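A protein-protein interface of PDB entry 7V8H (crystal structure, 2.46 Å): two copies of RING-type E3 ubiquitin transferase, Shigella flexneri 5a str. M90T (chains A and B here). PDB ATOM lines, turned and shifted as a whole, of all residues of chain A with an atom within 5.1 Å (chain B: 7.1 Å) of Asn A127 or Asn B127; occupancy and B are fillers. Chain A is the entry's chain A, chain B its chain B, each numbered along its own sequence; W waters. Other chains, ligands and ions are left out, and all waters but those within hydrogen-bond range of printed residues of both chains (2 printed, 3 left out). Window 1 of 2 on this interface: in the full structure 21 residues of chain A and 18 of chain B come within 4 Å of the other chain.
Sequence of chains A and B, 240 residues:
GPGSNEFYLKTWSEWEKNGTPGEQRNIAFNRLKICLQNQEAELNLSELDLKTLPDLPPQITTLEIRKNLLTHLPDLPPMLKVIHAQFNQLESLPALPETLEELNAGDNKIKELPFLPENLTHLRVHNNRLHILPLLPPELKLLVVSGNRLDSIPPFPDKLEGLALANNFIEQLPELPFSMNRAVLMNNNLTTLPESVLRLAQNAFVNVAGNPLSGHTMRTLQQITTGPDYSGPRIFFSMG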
ATOM      1  N   GLY A 106      20.326  -5.294 -11.748  1.00  0.00           N
ATOM      2  CA  GLY A 106      19.190  -5.259 -12.660  1.00  0.00           C
ATOM      3  C   GLY A 106      17.946  -5.902 -12.063  1.00  0.00           C
ATOM      4  O   GLY A 106      18.021  -6.723 -11.159  1.00  0.00           O
ATOM      5  N   ASP A 107      16.760  -5.516 -12.569  1.00  0.00           N
ATOM      6  CA  ASP A 107      15.501  -6.135 -12.139  1.00  0.00           C
ATOM      7  C   ASP A 107      15.247  -5.907 -10.659  1.00  0.00           C
ATOM      8  O   ASP A 107      14.883  -6.815  -9.919  1.00  0.00           O
ATOM      9  CB  ASP A 107      15.490  -7.624 -12.503  1.00  0.00           C
ATOM     10  CG  ASP A 107      15.073  -7.875 -13.970  1.00  0.00           C
ATOM     11  OD1 ASP A 107      14.011  -7.345 -14.404  1.00  0.00           O
ATOM     12  OD2 ASP A 107      15.893  -8.423 -14.749  1.00  0.00           O
ATOM     13  N   ASN A 108      15.420  -4.662 -10.241  1.00  0.00           N
ATOM     14  CA  ASN A 108      15.014  -4.224  -8.918  1.00  0.00           C
ATOM     15  C   ASN A 108      14.055  -3.056  -9.070  1.00  0.00           C
ATOM     16  O   ASN A 108      13.445  -2.886 -10.128  1.00  0.00           O
ATOM     17  CB  ASN A 108      16.236  -3.845  -8.074  1.00  0.00           C
ATOM     18  CG  ASN A 108      16.939  -5.051  -7.528  1.00  0.00           C
ATOM     19  OD1 ASN A 108      16.445  -5.678  -6.602  1.00  0.00           O
ATOM     20  ND2 ASN A 108      18.091  -5.403  -8.115  1.00  0.00           N
ATOM     21  N   VAL A 125      22.438  -2.355 -14.704  1.00  0.00           N
ATOM     22  CA  VAL A 125      21.335  -1.982 -13.838  1.00  0.00           C
ATOM     23  C   VAL A 125      20.036  -1.840 -14.648  1.00  0.00           C
ATOM     24  O   VAL A 125      19.228  -0.935 -14.410  1.00  0.00           O
ATOM     25  CB  VAL A 125      21.753  -0.718 -13.045  1.00  0.00           C
ATOM     26  CG1 VAL A 125      21.745   0.538 -13.901  1.00  0.00           C
ATOM     27  CG2 VAL A 125      20.957  -0.546 -11.778  1.00  0.00           C
ATOM     28  N   HIS A 126      19.786  -2.771 -15.576  1.00  0.00           N
ATOM     29  CA  HIS A 126      18.558  -2.658 -16.350  1.00  0.00           C
ATOM     30  C   HIS A 126      17.324  -3.081 -15.545  1.00  0.00           C
ATOM     31  O   HIS A 126      17.409  -3.770 -14.523  1.00  0.00           O
ATOM     32  CB  HIS A 126      18.557  -3.480 -17.640  1.00  0.00           C
ATOM     33  CG  HIS A 126      18.794  -4.945 -17.453  1.00  0.00           C
ATOM     34  ND1 HIS A 126      17.917  -5.761 -16.774  1.00  0.00           N
ATOM     35  CD2 HIS A 126      19.633  -5.780 -18.109  1.00  0.00           C
ATOM     36  CE1 HIS A 126      18.340  -7.010 -16.843  1.00  0.00           C
ATOM     37  NE2 HIS A 126      19.357  -7.053 -17.680  1.00  0.00           N
ATOM     38  N   ASN A 127      16.163  -2.667 -16.051  1.00  0.00           N
ATOM     39  CA  ASN A 127      14.855  -2.975 -15.476  1.00  0.00           C
ATOM     40  C   ASN A 127      14.749  -2.465 -14.040  1.00  0.00           C
ATOM     41  O   ASN A 127      14.351  -3.186 -13.127  1.00  0.00           O
ATOM     42  CB  ASN A 127      14.549  -4.465 -15.554  1.00  0.00           C
ATOM     43  CG  ASN A 127      14.393  -4.950 -16.977  1.00  0.00           C
ATOM     44  OD1 ASN A 127      14.000  -4.192 -17.856  1.00  0.00           O
ATOM     45  ND2 ASN A 127      14.700  -6.223 -17.214  1.00  0.00           N
ATOM     46  N   ASN A 128      15.119  -1.204 -13.848  1.00  0.00           N
ATOM     47  CA  ASN A 128      14.877  -0.506 -12.598  1.00  0.00           C
ATOM     48  C   ASN A 128      14.017   0.703 -12.917  1.00  0.00           C
ATOM     49  O   ASN A 128      13.318   0.705 -13.926  1.00  0.00           O
ATOM     50  CB  ASN A 128      16.201  -0.110 -11.940  1.00  0.00           C
ATOM     51  CG  ASN A 128      16.832  -1.256 -11.218  1.00  0.00           C
ATOM     52  OD1 ASN A 128      16.442  -1.569 -10.102  1.00  0.00           O
ATOM     53  ND2 ASN A 128      17.793  -1.916 -11.856  1.00  0.00           N
ATOM     54  N   ARG A 129      14.090   1.746 -12.102  1.00  0.00           N
ATOM     55  CA  ARG A 129      13.241   2.921 -12.248  1.00  0.00           C
ATOM     56  C   ARG A 129      14.077   4.192 -12.259  1.00  0.00           C
ATOM     57  O   ARG A 129      13.640   5.245 -11.792  1.00  0.00           O
ATOM     58  CB  ARG A 129      12.209   2.945 -11.124  1.00  0.00           C
ATOM     59  CG  ARG A 129      11.400   1.644 -11.089  1.00  0.00           C
ATOM     60  CD  ARG A 129      10.379   1.491  -9.968  1.00  0.00           C
ATOM     61  NE  ARG A 129       9.645   0.260 -10.246  1.00  0.00           N
ATOM     62  CZ  ARG A 129       8.705  -0.288  -9.483  1.00  0.00           C
ATOM     63  NH1 ARG A 129       8.333   0.270  -8.346  1.00  0.00           N
ATOM     64  NH2 ARG A 129       8.138  -1.408  -9.881  1.00  0.00           N
ATOM     65  N   SER A 146      19.316  -0.369 -19.830  1.00  0.00           N
ATOM     66  CA  SER A 146      18.110  -0.527 -20.632  1.00  0.00           C
ATOM     67  C   SER A 146      16.873  -0.601 -19.739  1.00  0.00           C
ATOM     68  O   SER A 146      16.945  -1.041 -18.592  1.00  0.00           O
ATOM     69  CB  SER A 146      18.241  -1.795 -21.487  1.00  0.00           C
ATOM     70  OG  SER A 146      19.496  -1.781 -22.181  1.00  0.00           O
ATOM     71  N   GLY A 147      15.728  -0.171 -20.268  1.00  0.00           N
ATOM     72  CA  GLY A 147      14.462  -0.378 -19.575  1.00  0.00           C
ATOM     73  C   GLY A 147      14.307   0.372 -18.266  1.00  0.00           C
ATOM     74  O   GLY A 147      13.806  -0.189 -17.283  1.00  0.00           O
ATOM     75  N   ASN A 148      14.725   1.631 -18.224  1.00  0.00           N
ATOM     76  CA  ASN A 148      14.538   2.459 -17.042  1.00  0.00           C
ATOM     77  C   ASN A 148      13.667   3.639 -17.459  1.00  0.00           C
ATOM     78  O   ASN A 148      12.892   3.519 -18.417  1.00  0.00           O
ATOM     79  CB  ASN A 148      15.888   2.902 -16.482  1.00  0.00           C
ATOM     80  CG  ASN A 148      16.553   1.835 -15.598  1.00  0.00           C
ATOM     81  OD1 ASN A 148      16.304   1.769 -14.400  1.00  0.00           O
ATOM     82  ND2 ASN A 148      17.397   1.016 -16.189  1.00  0.00           N
ATOM     83  N   ASN A 167      15.177   1.390 -24.658  1.00  0.00           N
ATOM     84  CA  ASN A 167      13.912   1.513 -23.960  1.00  0.00           C
ATOM     85  C   ASN A 167      14.040   2.471 -22.773  1.00  0.00           C
ATOM     86  O   ASN A 167      13.788   2.132 -21.621  1.00  0.00           O
ATOM     87  CB  ASN A 167      13.413   0.126 -23.546  1.00  0.00           C
ATOM     88  CG  ASN A 167      13.222  -0.797 -24.746  1.00  0.00           C
ATOM     89  OD1 ASN A 167      12.434  -0.511 -25.628  1.00  0.00           O
ATOM     90  ND2 ASN A 167      13.922  -1.905 -24.769  1.00  0.00           N
ATOM     91  N   PHE B  87       5.637   4.169 -24.079  1.00  0.00           N
ATOM     92  CA  PHE B  87       6.534   5.282 -23.748  1.00  0.00           C
ATOM     93  C   PHE B  87       5.744   6.526 -23.322  1.00  0.00           C
ATOM     94  O   PHE B  87       5.756   7.561 -23.977  1.00  0.00           O
ATOM     95  CB  PHE B  87       7.496   5.587 -24.915  1.00  0.00           C
ATOM     96  CG  PHE B  87       8.432   4.467 -25.210  1.00  0.00           C
ATOM     97  CD1 PHE B  87       9.579   4.295 -24.465  1.00  0.00           C
ATOM     98  CD2 PHE B  87       8.140   3.547 -26.193  1.00  0.00           C
ATOM     99  CE1 PHE B  87      10.440   3.229 -24.722  1.00  0.00           C
ATOM    100  CE2 PHE B  87       8.986   2.481 -26.451  1.00  0.00           C
ATOM    101  CZ  PHE B  87      10.139   2.319 -25.715  1.00  0.00           C
ATOM    102  N   ALA B 105       1.048  -0.797 -24.401  1.00  0.00           N
ATOM    103  CA  ALA B 105       1.289   0.182 -23.345  1.00  0.00           C
ATOM    104  C   ALA B 105       2.610  -0.086 -22.637  1.00  0.00           C
ATOM    105  O   ALA B 105       2.749   0.219 -21.445  1.00  0.00           O
ATOM    106  CB  ALA B 105       0.143   0.188 -22.330  1.00  0.00           C
ATOM    107  N   GLY B 106       3.591  -0.658 -23.352  1.00  0.00           N
ATOM    108  CA  GLY B 106       4.887  -0.898 -22.756  1.00  0.00           C
ATOM    109  C   GLY B 106       5.613   0.383 -22.384  1.00  0.00           C
ATOM    110  O   GLY B 106       5.366   1.475 -22.907  1.00  0.00           O
ATOM    111  N   ASP B 107       6.540   0.247 -21.442  1.00  0.00           N
ATOM    112  CA  ASP B 107       7.386   1.361 -21.023  1.00  0.00           C
ATOM    113  C   ASP B 107       6.525   2.478 -20.432  1.00  0.00           C
ATOM    114  O   ASP B 107       6.642   3.650 -20.788  1.00  0.00           O
ATOM    115  CB  ASP B 107       8.261   1.860 -22.179  1.00  0.00           C
ATOM    116  CG  ASP B 107       9.090   0.741 -22.817  1.00  0.00           C
ATOM    117  OD1 ASP B 107      10.108   0.331 -22.200  1.00  0.00           O
ATOM    118  OD2 ASP B 107       8.716   0.254 -23.932  1.00  0.00           O
ATOM    119  N   ASN B 108       5.631   2.089 -19.525  1.00  0.00           N
ATOM    120  CA  ASN B 108       4.892   3.026 -18.697  1.00  0.00           C
ATOM    121  C   ASN B 108       5.160   2.679 -17.233  1.00  0.00           C
ATOM    122  O   ASN B 108       6.134   1.976 -16.942  1.00  0.00           O
ATOM    123  CB  ASN B 108       3.401   2.976 -19.054  1.00  0.00           C
ATOM    124  CG  ASN B 108       3.081   3.819 -20.246  1.00  0.00           C
ATOM    125  OD1 ASN B 108       3.144   5.041 -20.173  1.00  0.00           O
ATOM    126  ND2 ASN B 108       2.759   3.184 -21.366  1.00  0.00           N
ATOM    127  N   LYS B 109       4.304   3.122 -16.308  1.00  0.00           N
ATOM    128  CA  LYS B 109       4.451   2.829 -14.884  1.00  0.00           C
ATOM    129  C   LYS B 109       3.221   2.115 -14.342  1.00  0.00           C
ATOM    130  O   LYS B 109       2.804   2.348 -13.204  1.00  0.00           O
ATOM    131  CB  LYS B 109       4.685   4.104 -14.074  1.00  0.00           C
ATOM    132  CG  LYS B 109       5.789   5.026 -14.564  1.00  0.00           C
ATOM    133  CD  LYS B 109       5.764   6.311 -13.736  1.00  0.00           C
ATOM    134  CE  LYS B 109       6.944   7.198 -14.047  1.00  0.00           C
ATOM    135  NZ  LYS B 109       6.918   8.436 -13.229  1.00  0.00           N
ATOM    136  N   ILE B 110       2.618   1.249 -15.146  1.00  0.00           N
ATOM    137  CA  ILE B 110       1.284   0.740 -14.846  1.00  0.00           C
ATOM    138  C   ILE B 110       1.402  -0.351 -13.792  1.00  0.00           C
ATOM    139  O   ILE B 110       2.130  -1.332 -13.978  1.00  0.00           O
ATOM    140  CB  ILE B 110       0.602   0.219 -16.123  1.00  0.00           C
ATOM    141  CG1 ILE B 110       0.285   1.382 -17.071  1.00  0.00           C
ATOM    142  CG2 ILE B 110      -0.647  -0.570 -15.780  1.00  0.00           C
ATOM    143  CD1 ILE B 110       0.054   0.958 -18.546  1.00  0.00           C
ATOM    144  N   VAL B 125       2.635  -5.175 -23.060  1.00  0.00           N
ATOM    145  CA  VAL B 125       2.810  -4.300 -21.894  1.00  0.00           C
ATOM    146  C   VAL B 125       4.128  -4.545 -21.160  1.00  0.00           C
ATOM    147  O   VAL B 125       4.151  -4.560 -19.919  1.00  0.00           O
ATOM    148  CB  VAL B 125       1.638  -4.459 -20.888  1.00  0.00           C
ATOM    149  CG1 VAL B 125       0.357  -3.909 -21.446  1.00  0.00           C
ATOM    150  CG2 VAL B 125       1.436  -5.939 -20.522  1.00  0.00           C
ATOM    151  N   HIS B 126       5.234  -4.709 -21.889  1.00  0.00           N
ATOM    152  CA  HIS B 126       6.495  -4.938 -21.191  1.00  0.00           C
ATOM    153  C   HIS B 126       7.005  -3.640 -20.546  1.00  0.00           C
ATOM    154  O   HIS B 126       6.573  -2.536 -20.885  1.00  0.00           O
ATOM    155  CB  HIS B 126       7.576  -5.528 -22.116  1.00  0.00           C
ATOM    156  CG  HIS B 126       7.964  -4.678 -23.302  1.00  0.00           C
ATOM    157  ND1 HIS B 126       8.292  -3.342 -23.203  1.00  0.00           N
ATOM    158  CD2 HIS B 126       8.204  -5.018 -24.593  1.00  0.00           C
ATOM    159  CE1 HIS B 126       8.642  -2.878 -24.390  1.00  0.00           C
ATOM    160  NE2 HIS B 126       8.601  -3.875 -25.252  1.00  0.00           N
ATOM    161  N   ASN B 127       7.925  -3.795 -19.580  1.00  0.00           N
ATOM    162  CA  ASN B 127       8.562  -2.664 -18.910  1.00  0.00           C
ATOM    163  C   ASN B 127       7.529  -1.762 -18.229  1.00  0.00           C
ATOM    164  O   ASN B 127       7.485  -0.552 -18.450  1.00  0.00           O
ATOM    165  CB  ASN B 127       9.428  -1.869 -19.891  1.00  0.00           C
ATOM    166  CG  ASN B 127      10.583  -2.694 -20.440  1.00  0.00           C
ATOM    167  OD1 ASN B 127      10.984  -3.701 -19.852  1.00  0.00           O
ATOM    168  ND2 ASN B 127      11.096  -2.292 -21.589  1.00  0.00           N
ATOM    169  N   ASN B 128       6.659  -2.379 -17.440  1.00  0.00           N
ATOM    170  CA  ASN B 128       5.753  -1.669 -16.546  1.00  0.00           C
ATOM    171  C   ASN B 128       6.024  -2.129 -15.121  1.00  0.00           C
ATOM    172  O   ASN B 128       7.128  -2.583 -14.814  1.00  0.00           O
ATOM    173  CB  ASN B 128       4.292  -1.905 -16.949  1.00  0.00           C
ATOM    174  CG  ASN B 128       3.853  -0.980 -18.070  1.00  0.00           C
ATOM    175  OD1 ASN B 128       3.531   0.181 -17.830  1.00  0.00           O
ATOM    176  ND2 ASN B 128       3.860  -1.481 -19.297  1.00  0.00           N
ATOM    177  N   ARG B 129       5.039  -2.057 -14.247  1.00  0.00           N
ATOM    178  CA  ARG B 129       5.259  -2.397 -12.847  1.00  0.00           C
ATOM    179  C   ARG B 129       4.222  -3.402 -12.369  1.00  0.00           C
ATOM    180  O   ARG B 129       3.868  -3.415 -11.191  1.00  0.00           O
ATOM    181  CB  ARG B 129       5.258  -1.134 -11.980  1.00  0.00           C
ATOM    182  CG  ARG B 129       6.019   0.016 -12.645  1.00  0.00           C
ATOM    183  CD  ARG B 129       6.484   1.083 -11.691  1.00  0.00           C
ATOM    184  NE  ARG B 129       7.427   2.002 -12.336  1.00  0.00           N
ATOM    185  CZ  ARG B 129       7.706   3.212 -11.869  1.00  0.00           C
ATOM    186  NH1 ARG B 129       7.112   3.637 -10.758  1.00  0.00           N
ATOM    187  NH2 ARG B 129       8.564   3.994 -12.508  1.00  0.00           N
ATOM    188  N   LEU B 130       3.754  -4.269 -13.272  1.00  0.00           N
ATOM    189  CA  LEU B 130       2.675  -5.201 -12.954  1.00  0.00           C
ATOM    190  C   LEU B 130       3.104  -6.247 -11.930  1.00  0.00           C
ATOM    191  O   LEU B 130       4.129  -6.916 -12.098  1.00  0.00           O
ATOM    192  CB  LEU B 130       2.192  -5.900 -14.227  1.00  0.00           C
ATOM    193  CG  LEU B 130       1.625  -4.938 -15.258  1.00  0.00           C
ATOM    194  CD1 LEU B 130       1.362  -5.620 -16.588  1.00  0.00           C
ATOM    195  CD2 LEU B 130       0.360  -4.312 -14.697  1.00  0.00           C
ATOM    196  N   VAL B 144       2.748 -10.125 -24.175  1.00  0.00           N
ATOM    197  CA  VAL B 144       4.123  -9.711 -23.858  1.00  0.00           C
ATOM    198  C   VAL B 144       4.083  -8.938 -22.542  1.00  0.00           C
ATOM    199  O   VAL B 144       3.477  -7.862 -22.471  1.00  0.00           O
ATOM    200  CB  VAL B 144       4.753  -8.851 -24.972  1.00  0.00           C
ATOM    201  CG1 VAL B 144       6.132  -8.346 -24.539  1.00  0.00           C
ATOM    202  CG2 VAL B 144       4.855  -9.613 -26.293  1.00  0.00           C
ATOM    203  N   VAL B 145       4.703  -9.489 -21.495  1.00  0.00           N
ATOM    204  CA  VAL B 145       4.678  -8.882 -20.164  1.00  0.00           C
ATOM    205  C   VAL B 145       6.089  -8.890 -19.587  1.00  0.00           C
ATOM    206  O   VAL B 145       6.273  -8.844 -18.370  1.00  0.00           O
ATOM    207  CB  VAL B 145       3.702  -9.614 -19.218  1.00  0.00           C
ATOM    208  CG1 VAL B 145       2.282  -9.460 -19.657  1.00  0.00           C
ATOM    209  CG2 VAL B 145       4.034 -11.091 -19.181  1.00  0.00           C
ATOM    210  N   SER B 146       7.091  -8.953 -20.452  1.00  0.00           N
ATOM    211  CA  SER B 146       8.482  -8.942 -20.017  1.00  0.00           C
ATOM    212  C   SER B 146       8.805  -7.691 -19.207  1.00  0.00           C
ATOM    213  O   SER B 146       8.170  -6.655 -19.354  1.00  0.00           O
ATOM    214  CB  SER B 146       9.402  -9.002 -21.230  1.00  0.00           C
ATOM    215  OG  SER B 146       9.115 -10.165 -21.977  1.00  0.00           O
ATOM    216  N   GLY B 147       9.791  -7.798 -18.326  1.00  0.00           N
ATOM    217  CA  GLY B 147      10.233  -6.635 -17.594  1.00  0.00           C
ATOM    218  C   GLY B 147       9.178  -6.057 -16.669  1.00  0.00           C
ATOM    219  O   GLY B 147       8.994  -4.837 -16.642  1.00  0.00           O
ATOM    220  N   ASN B 148       8.448  -6.905 -15.948  1.00  0.00           N
ATOM    221  CA  ASN B 148       7.492  -6.445 -14.950  1.00  0.00           C
ATOM    222  C   ASN B 148       7.852  -7.016 -13.578  1.00  0.00           C
ATOM    223  O   ASN B 148       8.995  -7.431 -13.365  1.00  0.00           O
ATOM    224  CB  ASN B 148       6.080  -6.822 -15.376  1.00  0.00           C
ATOM    225  CG  ASN B 148       5.495  -5.807 -16.337  1.00  0.00           C
ATOM    226  OD1 ASN B 148       5.089  -4.735 -15.922  1.00  0.00           O
ATOM    227  ND2 ASN B 148       5.488  -6.121 -17.625  1.00  0.00           N
ATOM    228  N   ARG B 149       6.904  -7.059 -12.646  1.00  0.00           N
ATOM    229  CA  ARG B 149       7.130  -7.606 -11.312  1.00  0.00           C
ATOM    230  C   ARG B 149       6.227  -8.788 -11.048  1.00  0.00           C
ATOM    231  O   ARG B 149       5.725  -8.964  -9.937  1.00  0.00           O
ATOM    232  CB  ARG B 149       6.912  -6.553 -10.229  1.00  0.00           C
ATOM    233  CG  ARG B 149       7.673  -5.265 -10.458  1.00  0.00           C
ATOM    234  CD  ARG B 149       9.175  -5.433 -10.249  1.00  0.00           C
ATOM    235  NE  ARG B 149       9.488  -6.021  -8.945  1.00  0.00           N
ATOM    236  CZ  ARG B 149      10.716  -6.360  -8.541  1.00  0.00           C
ATOM    237  NH1 ARG B 149      11.768  -6.142  -9.328  1.00  0.00           N
ATOM    238  NH2 ARG B 149      10.904  -6.897  -7.339  1.00  0.00           N
ATOM    239  N   ALA B 166       9.635 -12.852 -20.041  1.00  0.00           N
ATOM    240  CA  ALA B 166      11.010 -12.803 -19.564  1.00  0.00           C
ATOM    241  C   ALA B 166      11.198 -11.725 -18.508  1.00  0.00           C
ATOM    242  O   ALA B 166      10.599 -10.657 -18.579  1.00  0.00           O
ATOM    243  CB  ALA B 166      11.950 -12.497 -20.731  1.00  0.00           C
ATOM    244  N   ASN B 167      12.098 -11.983 -17.560  1.00  0.00           N
ATOM    245  CA  ASN B 167      12.505 -10.998 -16.560  1.00  0.00           C
ATOM    246  C   ASN B 167      11.336 -10.604 -15.671  1.00  0.00           C
ATOM    247  O   ASN B 167      10.926  -9.447 -15.618  1.00  0.00           O
ATOM    248  CB  ASN B 167      13.104  -9.757 -17.214  1.00  0.00           C
ATOM    249  CG  ASN B 167      14.320 -10.076 -18.032  1.00  0.00           C
ATOM    250  OD1 ASN B 167      15.340 -10.507 -17.507  1.00  0.00           O
ATOM    251  ND2 ASN B 167      14.225  -9.857 -19.329  1.00  0.00           N
ATOM    252  N   ASN B 168      10.775 -11.608 -15.011  1.00  0.00           N
ATOM    253  CA  ASN B 168       9.772 -11.406 -13.976  1.00  0.00           C
ATOM    254  C   ASN B 168      10.207 -12.268 -12.795  1.00  0.00           C
ATOM    255  O   ASN B 168      11.368 -12.686 -12.702  1.00  0.00           O
ATOM    256  CB  ASN B 168       8.382 -11.762 -14.504  1.00  0.00           C
ATOM    257  CG  ASN B 168       7.809 -10.687 -15.386  1.00  0.00           C
ATOM    258  OD1 ASN B 168       7.373  -9.660 -14.891  1.00  0.00           O
ATOM    259  ND2 ASN B 168       7.772 -10.930 -16.698  1.00  0.00           N
HETATM  260  O   HOH W   1       9.941  -1.681 -27.190  1.00  0.00           O
HETATM  261  O   HOH W   2      12.299  -5.087 -11.759  1.00  0.00           O
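Printed residues of chain A that touch a printed residue of chain B: Asp A107, Asn A108, Asn A127, Arg A129 and Asn A167.
Among the printed residues, 10 pairs touch across the chains.
Among the printed residues, no Asp or Glu carboxylate lies within 4 Å of a Lys or Arg side-chain nitrogen of the other chain.
The backbone carbonyl oxygen (O) of Asp A107 lies within hydrogen-bond range of the guanidinium group (NH1) of Arg B149.
Water W2 lies within hydrogen-bond range of NH1 of Arg B149, O of Asn A108 and O of Asn A127.
Water W1 bridges OD1 of Asn A167 (3.2 Å) and NE2 of His B126 (3.2 Å).
Asn A127 touches just these residues of chain B: Asn B127 (3.6 Å) and Asn B167 (3.9 Å).
Of the printed residues of chain A, Phe B87 touches Asn A167.
Asn B127 touches just these residues of chain A: Asn A127 (3.6 Å) and Asn A167 (3.9 Å).
Printed residues of chain A within 4 Å of Arg B129: Arg A129.
Printed residues of chain A within 4 Å of Arg B149: Asp A107 (3.2 Å), Asn A108 (3.7 Å) and Arg A129 (3.9 Å).
The nearest residue of chain A that does not touch Asn B127 is Gly A147 (4.4 Å).
The nearest printed residue of chain B that does not touch Asn A167 is His B126 (4.6 Å).
Among the printed residues, pairs that only touch across the chains: Arg A129 with Arg B129 (3.4 Å), Asp A107 with Asn B167 (3.5 Å), Asn A167 with Asp B107 (3.6 Å), Asn A167 with Phe B87 (3.6 Å), Asn A127 with Asn B127 (3.6 Å), Asn A108 with Arg B149 (3.7 Å), Asn A127 with Asn B167 (3.9 Å), Asn A167 with Asn B127 (3.9 Å) and Arg A129 with Arg B149 (3.9 Å).
Asp A107 touches Asn B167, and with the chains exchanged Asn A167 touches Asp B107.
Asn A127 touches its own counterpart, Asn B127.
Asn A127 touches Asn B167, and with the chains exchanged Asn A167 touches Asn B127.
Arg A129 touches its own counterpart, Arg B129.
Positions printed for both chains: 106, 107, 108, 125, 126, 127, 128, 129, 146, 147, 148 and 167.
O of Ile B110 is in hydrogen-bond range of N of Arg B129 (3.0 Å).
The backbone NH of Asn A127 lies within hydrogen-bond range of the backbone carbonyl oxygen of Ser A146 (3.1 Å).
N of Arg B129 lies within hydrogen-bond range of OD1 of Asn B148 (3.2 Å).
ND2 of Asn A108 sits at hydrogen-bond distance from O of Gly A106 (3.3 Å).
The backbone NH (N) of Asp A107 lies within hydrogen-bond range of the backbone carbonyl oxygen (O) of His A126.
The backbone NH (N) of Asn B127 lies within hydrogen-bond range of the backbone carbonyl oxygen (O) of Ser B146.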
